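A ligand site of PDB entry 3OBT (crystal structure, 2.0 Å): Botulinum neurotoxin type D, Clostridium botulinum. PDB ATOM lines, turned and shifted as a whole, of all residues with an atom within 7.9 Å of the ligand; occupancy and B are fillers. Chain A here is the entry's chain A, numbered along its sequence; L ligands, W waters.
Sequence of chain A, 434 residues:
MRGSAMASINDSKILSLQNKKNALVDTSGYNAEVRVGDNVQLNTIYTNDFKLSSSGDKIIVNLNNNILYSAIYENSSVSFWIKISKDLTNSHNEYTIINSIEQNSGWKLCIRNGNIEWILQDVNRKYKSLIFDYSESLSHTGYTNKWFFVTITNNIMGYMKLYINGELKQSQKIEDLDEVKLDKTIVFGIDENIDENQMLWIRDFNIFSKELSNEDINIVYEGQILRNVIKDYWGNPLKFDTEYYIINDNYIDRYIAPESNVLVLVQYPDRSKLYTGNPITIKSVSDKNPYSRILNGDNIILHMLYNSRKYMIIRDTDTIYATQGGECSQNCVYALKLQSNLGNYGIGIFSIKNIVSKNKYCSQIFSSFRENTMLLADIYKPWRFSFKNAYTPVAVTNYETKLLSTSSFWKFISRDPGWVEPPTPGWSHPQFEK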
ATOM      1  N   GLU A 259       4.592  23.987   8.823  1.00  0.00           N
ATOM      2  CA  GLU A 259       4.884  25.395   8.587  1.00  0.00           C
ATOM      3  C   GLU A 259       3.876  25.818   7.562  1.00  0.00           C
ATOM      4  O   GLU A 259       3.894  25.317   6.427  1.00  0.00           O
ATOM      5  CB  GLU A 259       6.328  25.581   8.041  1.00  0.00           C
ATOM      6  CG  GLU A 259       7.340  25.557   9.173  1.00  0.00           C
ATOM      7  CD  GLU A 259       8.740  25.694   8.638  1.00  0.00           C
ATOM      8  OE1 GLU A 259       8.924  25.946   7.425  1.00  0.00           O
ATOM      9  OE2 GLU A 259       9.662  25.597   9.466  1.00  0.00           O
ATOM     10  N   SER A 260       2.962  26.698   7.973  1.00  0.00           N
ATOM     11  CA  SER A 260       1.796  27.110   7.186  1.00  0.00           C
ATOM     12  C   SER A 260       1.047  25.841   6.755  1.00  0.00           C
ATOM     13  O   SER A 260       0.643  25.701   5.618  1.00  0.00           O
ATOM     14  CB  SER A 260       2.217  27.947   5.950  1.00  0.00           C
ATOM     15  OG  SER A 260       2.706  29.179   6.435  1.00  0.00           O
ATOM     16  N   ASN A 261       0.895  24.927   7.676  1.00  0.00           N
ATOM     17  CA  ASN A 261       0.136  23.704   7.430  1.00  0.00           C
ATOM     18  C   ASN A 261       0.666  22.845   6.297  1.00  0.00           C
ATOM     19  O   ASN A 261      -0.099  22.124   5.588  1.00  0.00           O
ATOM     20  CB  ASN A 261      -1.403  23.933   7.278  1.00  0.00           C
ATOM     21  CG  ASN A 261      -2.189  22.624   7.445  1.00  0.00           C
ATOM     22  OD1 ASN A 261      -1.779  21.768   8.215  1.00  0.00           O
ATOM     23  ND2 ASN A 261      -3.306  22.472   6.723  1.00  0.00           N
ATOM     24  N   VAL A 262       1.972  22.827   6.169  1.00  0.00           N
ATOM     25  CA  VAL A 262       2.638  21.913   5.277  1.00  0.00           C
ATOM     26  C   VAL A 262       3.715  21.269   6.173  1.00  0.00           C
ATOM     27  O   VAL A 262       4.519  22.008   6.823  1.00  0.00           O
ATOM     28  CB  VAL A 262       3.332  22.618   4.043  1.00  0.00           C
ATOM     29  CG1 VAL A 262       4.228  21.615   3.258  1.00  0.00           C
ATOM     30  CG2 VAL A 262       2.325  23.281   3.063  1.00  0.00           C
ATOM     31  N   ILE A 314      -2.604  14.020   7.304  1.00  0.00           N
ATOM     32  CA  ILE A 314      -3.252  13.534   6.091  1.00  0.00           C
ATOM     33  C   ILE A 314      -2.429  13.882   4.865  1.00  0.00           C
ATOM     34  O   ILE A 314      -1.664  14.851   4.868  1.00  0.00           O
ATOM     35  CB  ILE A 314      -4.661  14.131   5.925  1.00  0.00           C
ATOM     36  CG1 ILE A 314      -4.599  15.659   5.897  1.00  0.00           C
ATOM     37  CG2 ILE A 314      -5.580  13.642   7.038  1.00  0.00           C
ATOM     38  CD1 ILE A 314      -5.805  16.313   5.268  1.00  0.00           C
ATOM     39  N   ARG A 315      -2.589  13.092   3.811  1.00  0.00           N
ATOM     40  CA  ARG A 315      -1.931  13.370   2.544  1.00  0.00           C
ATOM     41  C   ARG A 315      -2.614  14.548   1.887  1.00  0.00           C
ATOM     42  O   ARG A 315      -3.798  14.800   2.117  1.00  0.00           O
ATOM     43  CB  ARG A 315      -1.999  12.149   1.633  1.00  0.00           C
ATOM     44  CG  ARG A 315      -0.917  12.107   0.556  1.00  0.00           C
ATOM     45  CD  ARG A 315      -1.409  11.380  -0.682  1.00  0.00           C
ATOM     46  NE  ARG A 315      -2.425  12.142  -1.400  1.00  0.00           N
ATOM     47  CZ  ARG A 315      -3.186  11.640  -2.373  1.00  0.00           C
ATOM     48  NH1 ARG A 315      -4.080  12.408  -2.970  1.00  0.00           N
ATOM     49  NH2 ARG A 315      -3.049  10.378  -2.745  1.00  0.00           N
ATOM     50  N   ASP A 316      -1.878  15.285   1.067  1.00  0.00           N
ATOM     51  CA  ASP A 316      -2.459  16.405   0.334  1.00  0.00           C
ATOM     52  C   ASP A 316      -3.412  15.862  -0.714  1.00  0.00           C
ATOM     53  O   ASP A 316      -3.216  14.771  -1.240  1.00  0.00           O
ATOM     54  CB  ASP A 316      -1.358  17.239  -0.331  1.00  0.00           C
ATOM     55  CG  ASP A 316      -0.837  18.331   0.579  1.00  0.00           C
ATOM     56  OD1 ASP A 316      -1.149  18.299   1.789  1.00  0.00           O
ATOM     57  OD2 ASP A 316      -0.111  19.221   0.077  1.00  0.00           O
ATOM     58  N   THR A 317      -4.463  16.620  -1.007  1.00  0.00           N
ATOM     59  CA  THR A 317      -5.430  16.221  -2.021  1.00  0.00           C
ATOM     60  C   THR A 317      -4.774  16.259  -3.399  1.00  0.00           C
ATOM     61  O   THR A 317      -4.949  15.348  -4.204  1.00  0.00           O
ATOM     62  CB  THR A 317      -6.670  17.125  -2.012  1.00  0.00           C
ATOM     63  OG1 THR A 317      -7.338  17.012  -0.751  1.00  0.00           O
ATOM     64  CG2 THR A 317      -7.633  16.720  -3.125  1.00  0.00           C
ATOM     65  N   ASP A 318      -4.004  17.310  -3.656  1.00  0.00           N
ATOM     66  CA  ASP A 318      -3.396  17.507  -4.960  1.00  0.00           C
ATOM     67  C   ASP A 318      -1.897  17.394  -5.009  1.00  0.00           C
ATOM     68  O   ASP A 318      -1.209  17.652  -4.023  1.00  0.00           O
ATOM     69  CB  ASP A 318      -3.838  18.861  -5.560  1.00  0.00           C
ATOM     70  CG  ASP A 318      -5.322  18.892  -5.937  1.00  0.00           C
ATOM     71  OD1 ASP A 318      -5.746  18.100  -6.803  1.00  0.00           O
ATOM     72  OD2 ASP A 318      -6.064  19.736  -5.367  1.00  0.00           O
ATOM     73  N   THR A 319      -1.392  16.992  -6.165  1.00  0.00           N
ATOM     74  CA  THR A 319       0.033  16.903  -6.335  1.00  0.00           C
ATOM     75  C   THR A 319       0.632  18.265  -6.030  1.00  0.00           C
ATOM     76  O   THR A 319      -0.078  19.255  -5.832  1.00  0.00           O
ATOM     77  CB  THR A 319       0.455  16.445  -7.744  1.00  0.00           C
ATOM     78  OG1 THR A 319       0.023  17.401  -8.722  1.00  0.00           O
ATOM     79  CG2 THR A 319      -0.127  15.081  -8.057  1.00  0.00           C
ATOM     80  N   ILE A 320       1.955  18.291  -5.988  1.00  0.00           N
ATOM     81  CA  ILE A 320       2.714  19.396  -5.444  1.00  0.00           C
ATOM     82  C   ILE A 320       2.963  20.542  -6.438  1.00  0.00           C
ATOM     83  O   ILE A 320       2.931  21.716  -6.046  1.00  0.00           O
ATOM     84  CB  ILE A 320       4.003  18.850  -4.786  1.00  0.00           C
ATOM     85  CG1 ILE A 320       4.783  19.938  -4.052  1.00  0.00           C
ATOM     86  CG2 ILE A 320       4.838  18.091  -5.814  1.00  0.00           C
ATOM     87  CD1 ILE A 320       5.693  19.367  -2.971  1.00  0.00           C
ATOM     88  N   ALA A 322       0.844  20.956  -8.904  1.00  0.00           N
ATOM     89  CA  ALA A 322      -0.451  20.945  -9.559  1.00  0.00           C
ATOM     90  C   ALA A 322      -0.865  22.351  -9.987  1.00  0.00           C
ATOM     91  O   ALA A 322      -0.458  23.340  -9.379  1.00  0.00           O
ATOM     92  CB  ALA A 322      -1.507  20.352  -8.618  1.00  0.00           C
ATOM     93  N   TYR A 334       2.964  14.210  -3.500  1.00  0.00           N
ATOM     94  CA  TYR A 334       2.053  14.929  -2.585  1.00  0.00           C
ATOM     95  C   TYR A 334       2.756  15.314  -1.273  1.00  0.00           C
ATOM     96  O   TYR A 334       3.309  14.414  -0.589  1.00  0.00           O
ATOM     97  CB  TYR A 334       0.867  14.028  -2.196  1.00  0.00           C
ATOM     98  CG  TYR A 334       0.077  13.517  -3.415  1.00  0.00           C
ATOM     99  CD1 TYR A 334      -1.067  14.179  -3.842  1.00  0.00           C
ATOM    100  CD2 TYR A 334       0.495  12.386  -4.113  1.00  0.00           C
ATOM    101  CE1 TYR A 334      -1.767  13.751  -4.948  1.00  0.00           C
ATOM    102  CE2 TYR A 334      -0.244  11.914  -5.221  1.00  0.00           C
ATOM    103  CZ  TYR A 334      -1.353  12.616  -5.634  1.00  0.00           C
ATOM    104  OH  TYR A 334      -2.095  12.175  -6.731  1.00  0.00           O
ATOM    105  N   ALA A 335       2.628  16.591  -0.867  1.00  0.00           N
ATOM    106  CA  ALA A 335       3.110  17.051   0.443  1.00  0.00           C
ATOM    107  C   ALA A 335       2.072  16.564   1.441  1.00  0.00           C
ATOM    108  O   ALA A 335       1.033  16.008   1.021  1.00  0.00           O
ATOM    109  CB  ALA A 335       3.263  18.607   0.474  1.00  0.00           C
ATOM    110  N   LEU A 336       2.323  16.738   2.754  1.00  0.00           N
ATOM    111  CA  LEU A 336       1.406  16.353   3.810  1.00  0.00           C
ATOM    112  C   LEU A 336       0.956  17.535   4.654  1.00  0.00           C
ATOM    113  O   LEU A 336       1.630  18.571   4.709  1.00  0.00           O
ATOM    114  CB  LEU A 336       2.041  15.337   4.796  1.00  0.00           C
ATOM    115  CG  LEU A 336       2.787  14.134   4.171  1.00  0.00           C
ATOM    116  CD1 LEU A 336       3.511  13.257   5.191  1.00  0.00           C
ATOM    117  CD2 LEU A 336       1.818  13.243   3.324  1.00  0.00           C
ATOM    118  N   LYS A 337      -0.171  17.351   5.345  1.00  0.00           N
ATOM    119  CA  LYS A 337      -0.688  18.413   6.105  1.00  0.00           C
ATOM    120  C   LYS A 337      -1.396  17.906   7.319  1.00  0.00           C
ATOM    121  O   LYS A 337      -1.478  16.682   7.554  1.00  0.00           O
ATOM    122  CB  LYS A 337      -1.582  19.326   5.270  1.00  0.00           C
ATOM    123  CG  LYS A 337      -2.936  18.728   4.886  1.00  0.00           C
ATOM    124  CD  LYS A 337      -3.563  19.581   3.710  1.00  0.00           C
ATOM    125  CE  LYS A 337      -4.989  19.072   3.345  1.00  0.00           C
ATOM    126  NZ  LYS A 337      -5.577  19.890   2.205  1.00  0.00           N
ATOM    127  N   LEU A 338      -1.918  18.855   8.090  1.00  0.00           N
ATOM    128  CA  LEU A 338      -2.589  18.490   9.327  1.00  0.00           C
ATOM    129  C   LEU A 338      -4.103  18.800   9.249  1.00  0.00           C
ATOM    130  O   LEU A 338      -4.502  19.748   8.568  1.00  0.00           O
ATOM    131  CB  LEU A 338      -2.015  19.283  10.496  1.00  0.00           C
ATOM    132  CG  LEU A 338      -0.584  18.951  10.954  1.00  0.00           C
ATOM    133  CD1 LEU A 338      -0.201  19.732  12.215  1.00  0.00           C
ATOM    134  CD2 LEU A 338      -0.378  17.380  11.130  1.00  0.00           C
ATOM    135  N   ILE A 347      -7.773   9.341   3.378  1.00  0.00           N
ATOM    136  CA  ILE A 347      -6.638  10.192   3.029  1.00  0.00           C
ATOM    137  C   ILE A 347      -5.615  10.270   4.165  1.00  0.00           C
ATOM    138  O   ILE A 347      -4.475  10.697   3.965  1.00  0.00           O
ATOM    139  CB  ILE A 347      -7.098  11.590   2.537  1.00  0.00           C
ATOM    140  CG1 ILE A 347      -5.982  12.276   1.757  1.00  0.00           C
ATOM    141  CG2 ILE A 347      -7.551  12.459   3.707  1.00  0.00           C
ATOM    142  CD1 ILE A 347      -6.444  13.472   0.956  1.00  0.00           C
ATOM    143  N   PRO A 382       7.074  22.963  -1.472  1.00  0.00           N
ATOM    144  CA  PRO A 382       5.791  22.394  -1.046  1.00  0.00           C
ATOM    145  C   PRO A 382       4.688  23.416  -0.800  1.00  0.00           C
ATOM    146  O   PRO A 382       3.546  23.022  -0.548  1.00  0.00           O
ATOM    147  CB  PRO A 382       6.171  21.701   0.257  1.00  0.00           C
ATOM    148  CG  PRO A 382       7.215  22.602   0.837  1.00  0.00           C
ATOM    149  CD  PRO A 382       7.985  23.170  -0.335  1.00  0.00           C
ATOM    150  N   TRP A 383       5.003  24.709  -0.867  1.00  0.00           N
ATOM    151  CA  TRP A 383       4.009  25.743  -0.611  1.00  0.00           C
ATOM    152  C   TRP A 383       3.393  26.282  -1.904  1.00  0.00           C
ATOM    153  O   TRP A 383       4.100  26.685  -2.823  1.00  0.00           O
ATOM    154  CB  TRP A 383       4.623  26.899   0.184  1.00  0.00           C
ATOM    155  CG  TRP A 383       4.968  26.532   1.598  1.00  0.00           C
ATOM    156  CD1 TRP A 383       4.103  26.345   2.631  1.00  0.00           C
ATOM    157  CD2 TRP A 383       6.284  26.306   2.121  1.00  0.00           C
ATOM    158  NE1 TRP A 383       4.785  26.022   3.774  1.00  0.00           N
ATOM    159  CE2 TRP A 383       6.131  25.979   3.490  1.00  0.00           C
ATOM    160  CE3 TRP A 383       7.566  26.337   1.575  1.00  0.00           C
ATOM    161  CZ2 TRP A 383       7.214  25.702   4.309  1.00  0.00           C
ATOM    162  CZ3 TRP A 383       8.645  26.052   2.391  1.00  0.00           C
ATOM    163  CH2 TRP A 383       8.464  25.743   3.746  1.00  0.00           C
ATOM    164  N   ARG A 384       2.066  26.289  -1.960  1.00  0.00           N
ATOM    165  CA  ARG A 384       1.351  26.747  -3.148  1.00  0.00           C
ATOM    166  C   ARG A 384       1.714  28.187  -3.512  1.00  0.00           C
ATOM    167  O   ARG A 384       1.866  28.505  -4.689  1.00  0.00           O
ATOM    168  CB  ARG A 384      -0.153  26.627  -2.937  1.00  0.00           C
ATOM    169  CG  ARG A 384      -0.619  25.233  -2.583  1.00  0.00           C
ATOM    170  CD  ARG A 384      -1.217  24.518  -3.789  1.00  0.00           C
ATOM    171  NE  ARG A 384      -1.528  23.127  -3.505  1.00  0.00           N
ATOM    172  CZ  ARG A 384      -1.037  22.094  -4.191  1.00  0.00           C
ATOM    173  NH1 ARG A 384      -0.222  22.311  -5.219  1.00  0.00           N
ATOM    174  NH2 ARG A 384      -1.372  20.865  -3.856  1.00  0.00           N
ATOM    175  N   PHE A 385       1.831  29.046  -2.508  1.00  0.00           N
ATOM    176  CA  PHE A 385       2.032  30.467  -2.746  1.00  0.00           C
ATOM    177  C   PHE A 385       3.466  30.947  -2.511  1.00  0.00           C
ATOM    178  O   PHE A 385       3.692  32.068  -2.054  1.00  0.00           O
ATOM    179  CB  PHE A 385       1.054  31.281  -1.889  1.00  0.00           C
ATOM    180  CG  PHE A 385      -0.393  31.037  -2.234  1.00  0.00           C
ATOM    181  CD1 PHE A 385      -1.006  31.775  -3.236  1.00  0.00           C
ATOM    182  CD2 PHE A 385      -1.126  30.064  -1.579  1.00  0.00           C
ATOM    183  CE1 PHE A 385      -2.324  31.549  -3.575  1.00  0.00           C
ATOM    184  CE2 PHE A 385      -2.452  29.839  -1.913  1.00  0.00           C
ATOM    185  CZ  PHE A 385      -3.049  30.578  -2.907  1.00  0.00           C
HETATM  186  C1  LIG L   1      -3.886  19.939  -0.985  1.00  0.00           C
HETATM  187  C2  LIG L   1      -3.641  21.402  -0.787  1.00  0.00           C
HETATM  188  C3  LIG L   1      -2.196  21.717  -0.416  1.00  0.00           C
HETATM  189  C4  LIG L   1      -2.128  23.214  -0.044  1.00  0.00           C
HETATM  190  C5  LIG L   1      -3.215  23.640   0.934  1.00  0.00           C
HETATM  191  C6  LIG L   1      -4.601  23.307   0.336  1.00  0.00           C
HETATM  192  C7  LIG L   1      -5.795  23.556   1.273  1.00  0.00           C
HETATM  193  C8  LIG L   1      -7.059  22.956   0.633  1.00  0.00           C
HETATM  194  C9  LIG L   1      -8.394  23.136   1.359  1.00  0.00           C
HETATM  195  C10 LIG L   1      -2.734  25.811   2.236  1.00  0.00           C
HETATM  196  C11 LIG L   1      -2.852  27.305   2.028  1.00  0.00           C
HETATM  197  N1  LIG L   1      -3.148  25.149   1.089  1.00  0.00           N
HETATM  198  O1  LIG L   1      -3.593  19.516  -2.150  1.00  0.00           O
HETATM  199  O2  LIG L   1      -4.371  19.323   0.006  1.00  0.00           O
HETATM  200  O3  LIG L   1      -3.846  22.081  -2.036  1.00  0.00           O
HETATM  201  O4  LIG L   1      -0.812  23.445   0.591  1.00  0.00           O
HETATM  202  O5  LIG L   1      -4.672  21.871   0.117  1.00  0.00           O
HETATM  203  O6  LIG L   1      -5.558  22.823   2.466  1.00  0.00           O
HETATM  204  O7  LIG L   1      -7.270  23.715  -0.580  1.00  0.00           O
HETATM  205  O8  LIG L   1      -8.438  24.504   1.780  1.00  0.00           O
HETATM  206  O9  LIG L   1      -2.375  25.311   3.359  1.00  0.00           O
HETATM  207  O   HOH W   1      -1.237  22.107   3.184  1.00  0.00           O
HETATM  208  O   HOH W   2      -5.768  21.526  -3.704  1.00  0.00           O
HETATM  209  O   HOH W   3      -5.917  16.664   1.611  1.00  0.00           O
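The backbone NH of Thr 317 is in hydrogen-bond range of an oxygen (O2) of the ligand.
NH2 of Arg 384 is in salt-bridge range of O1 of the ligand (3.1 Å).
NZ of Lys 337 lies within salt-bridge range of O2 of the ligand.
The backbone NH (N) of Asp 318 is in hydrogen-bond range of an oxygen (O1) of the ligand, 2.7 Å away.
O of Ala 335 sits at hydrogen-bond distance from N of Asp 316, 3.0 Å away.
O of Thr 319 lies within hydrogen-bond range of NH2 of Arg 384 (2.9 Å).
O of Lys 337 sits at hydrogen-bond distance from N of Ile 314, at 2.9 Å.
NH2 of Arg 384 is in hydrogen-bond range of O of Asp 318 (3.2 Å).
The guanidinium group (NH1) of Arg 384 sits at hydrogen-bond distance from the backbone carbonyl oxygen (O) of Ile 320 (3.3 Å).
The guanidinium group (NH1) of Arg 315 is in hydrogen-bond range of the backbone carbonyl oxygen (O) of Thr 317 (3.3 Å).
Ser 260 touches the ligand (O to O9, 3.8 Å).
Val 262 touches the ligand (CG2 to O4, 3.997 Å).
Asp 316 touches the ligand (OD2 to C3, 3.3 Å).
Hydrophobic or aromatic side chains that line the ligand: Val 262.
The nearest printed residue that does not touch the ligand is Asn 261 (4.3 Å).
Water W2 bridges OD2 of Asp 318 (2.5 Å) and O3 of the ligand (2.6 Å).
Water W1 bridges O of Asn 261 (2.7 Å) and O4 of the ligand (2.9 Å).
Water W3 lies within hydrogen-bond range of OG1 of Thr 317 (2.8 Å), O of Arg 315 (2.9 Å), NZ of Lys 337 (3.3 Å) and O2 of the ligand (3.5 Å).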
